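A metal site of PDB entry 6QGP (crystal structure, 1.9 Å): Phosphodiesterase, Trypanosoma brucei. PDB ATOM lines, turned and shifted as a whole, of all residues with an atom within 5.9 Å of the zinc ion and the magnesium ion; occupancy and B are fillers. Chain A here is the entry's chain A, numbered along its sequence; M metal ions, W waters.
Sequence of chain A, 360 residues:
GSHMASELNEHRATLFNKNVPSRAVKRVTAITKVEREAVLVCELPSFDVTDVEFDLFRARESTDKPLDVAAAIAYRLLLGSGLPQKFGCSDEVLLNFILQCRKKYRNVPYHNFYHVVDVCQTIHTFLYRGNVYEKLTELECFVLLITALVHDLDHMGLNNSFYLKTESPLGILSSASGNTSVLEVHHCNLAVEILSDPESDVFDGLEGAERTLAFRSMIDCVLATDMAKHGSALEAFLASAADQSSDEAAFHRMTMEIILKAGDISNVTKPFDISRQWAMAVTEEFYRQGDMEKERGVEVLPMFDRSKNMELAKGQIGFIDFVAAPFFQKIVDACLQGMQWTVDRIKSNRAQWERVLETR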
ATOM      1  N   TYR A 110     -18.469 -13.382   2.463  1.00  0.00           N
ATOM      2  CA  TYR A 110     -17.316 -14.175   1.931  1.00  0.00           C
ATOM      3  C   TYR A 110     -17.642 -14.893   0.601  1.00  0.00           C
ATOM      4  O   TYR A 110     -16.942 -14.659  -0.390  1.00  0.00           O
ATOM      5  CB  TYR A 110     -16.834 -15.176   2.977  1.00  0.00           C
ATOM      6  CG  TYR A 110     -15.642 -15.938   2.478  1.00  0.00           C
ATOM      7  CD1 TYR A 110     -14.403 -15.345   2.494  1.00  0.00           C
ATOM      8  CD2 TYR A 110     -15.747 -17.211   1.956  1.00  0.00           C
ATOM      9  CE1 TYR A 110     -13.281 -15.987   2.010  1.00  0.00           C
ATOM     10  CE2 TYR A 110     -14.618 -17.885   1.473  1.00  0.00           C
ATOM     11  CZ  TYR A 110     -13.392 -17.252   1.489  1.00  0.00           C
ATOM     12  OH  TYR A 110     -12.242 -17.847   1.040  1.00  0.00           O
ATOM     13  N   HIS A 111     -18.665 -15.753   0.558  1.00  0.00           N
ATOM     14  CA  HIS A 111     -18.999 -16.587  -0.640  1.00  0.00           C
ATOM     15  C   HIS A 111     -19.790 -15.783  -1.665  1.00  0.00           C
ATOM     16  O   HIS A 111     -20.920 -16.199  -2.028  1.00  0.00           O
ATOM     17  CB  HIS A 111     -19.712 -17.870  -0.216  1.00  0.00           C
ATOM     18  CG  HIS A 111     -18.832 -18.816   0.499  1.00  0.00           C
ATOM     19  ND1 HIS A 111     -18.944 -19.016   1.856  1.00  0.00           N
ATOM     20  CD2 HIS A 111     -17.798 -19.576   0.075  1.00  0.00           C
ATOM     21  CE1 HIS A 111     -18.030 -19.878   2.241  1.00  0.00           C
ATOM     22  NE2 HIS A 111     -17.305 -20.238   1.163  1.00  0.00           N
ATOM     23  N   HIS A 115     -15.035 -13.648  -4.126  1.00  0.00           N
ATOM     24  CA  HIS A 115     -14.387 -14.954  -3.792  1.00  0.00           C
ATOM     25  C   HIS A 115     -14.089 -15.755  -5.058  1.00  0.00           C
ATOM     26  O   HIS A 115     -12.965 -16.324  -5.175  1.00  0.00           O
ATOM     27  CB  HIS A 115     -15.237 -15.768  -2.807  1.00  0.00           C
ATOM     28  CG  HIS A 115     -14.803 -17.190  -2.656  1.00  0.00           C
ATOM     29  ND1 HIS A 115     -13.543 -17.540  -2.190  1.00  0.00           N
ATOM     30  CD2 HIS A 115     -15.449 -18.348  -2.919  1.00  0.00           C
ATOM     31  CE1 HIS A 115     -13.433 -18.869  -2.169  1.00  0.00           C
ATOM     32  NE2 HIS A 115     -14.591 -19.386  -2.604  1.00  0.00           N
ATOM     33  N   VAL A 116     -15.035 -15.851  -5.981  1.00  0.00           N
ATOM     34  CA  VAL A 116     -14.881 -16.772  -7.150  1.00  0.00           C
ATOM     35  C   VAL A 116     -13.937 -16.099  -8.157  1.00  0.00           C
ATOM     36  O   VAL A 116     -13.114 -16.831  -8.777  1.00  0.00           O
ATOM     37  CB  VAL A 116     -16.246 -17.206  -7.734  1.00  0.00           C
ATOM     38  CG1 VAL A 116     -17.115 -17.833  -6.658  1.00  0.00           C
ATOM     39  CG2 VAL A 116     -17.014 -16.091  -8.428  1.00  0.00           C
ATOM     40  N   VAL A 119     -10.588 -16.801  -6.734  1.00  0.00           N
ATOM     41  CA  VAL A 119     -10.179 -18.224  -6.973  1.00  0.00           C
ATOM     42  C   VAL A 119      -9.685 -18.384  -8.408  1.00  0.00           C
ATOM     43  O   VAL A 119      -8.680 -19.092  -8.637  1.00  0.00           O
ATOM     44  CB  VAL A 119     -11.330 -19.186  -6.615  1.00  0.00           C
ATOM     45  CG1 VAL A 119     -11.025 -20.593  -7.110  1.00  0.00           C
ATOM     46  CG2 VAL A 119     -11.623 -19.182  -5.127  1.00  0.00           C
ATOM     47  N   HIS A 151     -18.111 -22.128  -9.148  1.00  0.00           N
ATOM     48  CA  HIS A 151     -17.927 -23.206  -8.151  1.00  0.00           C
ATOM     49  C   HIS A 151     -18.709 -22.931  -6.854  1.00  0.00           C
ATOM     50  O   HIS A 151     -18.765 -23.861  -6.036  1.00  0.00           O
ATOM     51  CB  HIS A 151     -16.437 -23.464  -7.897  1.00  0.00           C
ATOM     52  CG  HIS A 151     -15.873 -22.622  -6.798  1.00  0.00           C
ATOM     53  ND1 HIS A 151     -15.378 -21.354  -7.017  1.00  0.00           N
ATOM     54  CD2 HIS A 151     -15.737 -22.846  -5.477  1.00  0.00           C
ATOM     55  CE1 HIS A 151     -14.965 -20.829  -5.875  1.00  0.00           C
ATOM     56  NE2 HIS A 151     -15.152 -21.725  -4.922  1.00  0.00           N
ATOM     57  N   ASP A 152     -19.225 -21.704  -6.680  1.00  0.00           N
ATOM     58  CA  ASP A 152     -20.006 -21.324  -5.467  1.00  0.00           C
ATOM     59  C   ASP A 152     -21.305 -20.585  -5.852  1.00  0.00           C
ATOM     60  O   ASP A 152     -21.721 -19.702  -5.068  1.00  0.00           O
ATOM     61  CB  ASP A 152     -19.164 -20.501  -4.485  1.00  0.00           C
ATOM     62  CG  ASP A 152     -18.337 -21.354  -3.547  1.00  0.00           C
ATOM     63  OD1 ASP A 152     -18.759 -22.494  -3.260  1.00  0.00           O
ATOM     64  OD2 ASP A 152     -17.269 -20.879  -3.108  1.00  0.00           O
ATOM     65  N   HIS A 155     -24.575 -19.337  -3.379  1.00  0.00           N
ATOM     66  CA  HIS A 155     -24.181 -19.560  -1.955  1.00  0.00           C
ATOM     67  C   HIS A 155     -24.878 -18.513  -1.098  1.00  0.00           C
ATOM     68  O   HIS A 155     -24.874 -17.349  -1.505  1.00  0.00           O
ATOM     69  CB  HIS A 155     -22.662 -19.462  -1.793  1.00  0.00           C
ATOM     70  CG  HIS A 155     -22.157 -20.208  -0.620  1.00  0.00           C
ATOM     71  ND1 HIS A 155     -22.497 -19.855   0.657  1.00  0.00           N
ATOM     72  CD2 HIS A 155     -21.304 -21.256  -0.535  1.00  0.00           C
ATOM     73  CE1 HIS A 155     -21.914 -20.688   1.495  1.00  0.00           C
ATOM     74  NE2 HIS A 155     -21.148 -21.549   0.788  1.00  0.00           N
ATOM     75  N   GLU A 184     -22.599 -28.065  -3.140  1.00  0.00           N
ATOM     76  CA  GLU A 184     -21.786 -28.368  -4.346  1.00  0.00           C
ATOM     77  C   GLU A 184     -22.710 -28.874  -5.451  1.00  0.00           C
ATOM     78  O   GLU A 184     -22.570 -28.358  -6.579  1.00  0.00           O
ATOM     79  CB  GLU A 184     -20.621 -29.319  -4.021  1.00  0.00           C
ATOM     80  CG  GLU A 184     -19.581 -28.715  -3.065  1.00  0.00           C
ATOM     81  CD  GLU A 184     -20.003 -28.561  -1.606  1.00  0.00           C
ATOM     82  OE1 GLU A 184     -20.995 -29.252  -1.165  1.00  0.00           O
ATOM     83  OE2 GLU A 184     -19.355 -27.762  -0.897  1.00  0.00           O
ATOM     84  N   HIS A 187     -24.688 -25.933  -6.763  1.00  0.00           N
ATOM     85  CA  HIS A 187     -23.812 -25.053  -7.581  1.00  0.00           C
ATOM     86  C   HIS A 187     -23.686 -25.622  -8.992  1.00  0.00           C
ATOM     87  O   HIS A 187     -23.717 -24.830  -9.960  1.00  0.00           O
ATOM     88  CB  HIS A 187     -22.447 -24.877  -6.900  1.00  0.00           C
ATOM     89  CG  HIS A 187     -22.538 -24.368  -5.497  1.00  0.00           C
ATOM     90  ND1 HIS A 187     -23.383 -23.347  -5.135  1.00  0.00           N
ATOM     91  CD2 HIS A 187     -21.880 -24.748  -4.374  1.00  0.00           C
ATOM     92  CE1 HIS A 187     -23.257 -23.104  -3.848  1.00  0.00           C
ATOM     93  NE2 HIS A 187     -22.333 -23.950  -3.359  1.00  0.00           N
ATOM     94  N   THR A 225     -14.812 -29.667  -4.047  1.00  0.00           N
ATOM     95  CA  THR A 225     -14.634 -28.518  -3.126  1.00  0.00           C
ATOM     96  C   THR A 225     -15.325 -28.769  -1.768  1.00  0.00           C
ATOM     97  O   THR A 225     -15.078 -27.939  -0.864  1.00  0.00           O
ATOM     98  CB  THR A 225     -15.135 -27.190  -3.688  1.00  0.00           C
ATOM     99  OG1 THR A 225     -16.535 -27.221  -4.006  1.00  0.00           O
ATOM    100  CG2 THR A 225     -14.387 -26.767  -4.932  1.00  0.00           C
ATOM    101  N   ASP A 264      -9.476 -22.614  -3.673  1.00  0.00           N
ATOM    102  CA  ASP A 264     -10.556 -22.406  -2.694  1.00  0.00           C
ATOM    103  C   ASP A 264     -10.000 -22.219  -1.255  1.00  0.00           C
ATOM    104  O   ASP A 264     -10.662 -21.500  -0.508  1.00  0.00           O
ATOM    105  CB  ASP A 264     -11.575 -23.555  -2.739  1.00  0.00           C
ATOM    106  CG  ASP A 264     -12.973 -23.100  -2.352  1.00  0.00           C
ATOM    107  OD1 ASP A 264     -13.268 -21.937  -2.584  1.00  0.00           O
ATOM    108  OD2 ASP A 264     -13.737 -23.923  -1.830  1.00  0.00           O
HETATM  109 ZN    ZN M   1     -15.293 -21.427  -2.714  1.00  0.00          ZN
HETATM  110 MG    MG M   2     -17.931 -23.979  -2.034  1.00  0.00          MG
HETATM  111  O   HOH W   1     -15.232 -21.431  -0.689  1.00  0.00           O
HETATM  112  O   HOH W   2     -20.144 -24.025  -1.420  1.00  0.00           O
HETATM  113  O   HOH W   3     -17.305 -26.044  -1.249  1.00  0.00           O
HETATM  114  O   HOH W   4     -18.173 -25.267  -4.131  1.00  0.00           O
HETATM  115  O   HOH W   5     -16.008 -23.295  -2.019  1.00  0.00           O
HETATM  116  O   HOH W   6     -17.770 -22.955   0.197  1.00  0.00           O
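A ring nitrogen (ND1) of His 115 lies within hydrogen-bond range of the side-chain hydroxyl (OH) of Tyr 110 (3.5 Å).
Within 4 Å of the zinc ion: His 115, His 151, Asp 152 and Asp 264.
Of the 12 residues printed, 1 comes within 4 Å of the magnesium ion.
The nearest printed residue that does not touch the magnesium ion is Thr 225 (4.04 Å).
Water W1 binds the zinc ion, 2.0 Å away.
The zinc ion is bound by OD2 of Asp 152 (2.1 Å).
The zinc ion is bound by OD1 of Asp 264 (2.1 Å).
Water W5 binds the zinc ion.
The zinc ion is bound by NE2 of His 115, 2.2 Å away.
NE2 of His 151 is bound to the zinc ion (2.2 Å).
The zinc ion has six donor atoms within binding distance.
Water W5 is bound to the magnesium ion (2.0 Å).
OD1 of Asp 152 binds the magnesium ion (2.1 Å).
Water W3 binds the magnesium ion.
The magnesium ion is bound by water W2 (2.3 Å).
The magnesium ion is bound by water W6.
Water W4 binds the magnesium ion, 2.5 Å away.
Water W1 lies within hydrogen-bond range of a ring nitrogen (NE2) of His 111 (3.0 Å) and the side-chain carboxylate of Asp 264 (3.1 Å).
Water W4 bridges the backbone carbonyl oxygen of His 151 (2.4 Å) and the side-chain hydroxyl of Thr 225 (2.6 Å).
Water W2 lies within hydrogen-bond range of a ring nitrogen (NE2) of His 187 and a ring nitrogen (NE2) of His 155.
Water W3 bridges the side-chain carboxylate (OE2) of Glu 184 (2.7 Å) and the backbone carbonyl oxygen (O) of Thr 225 (2.9 Å).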
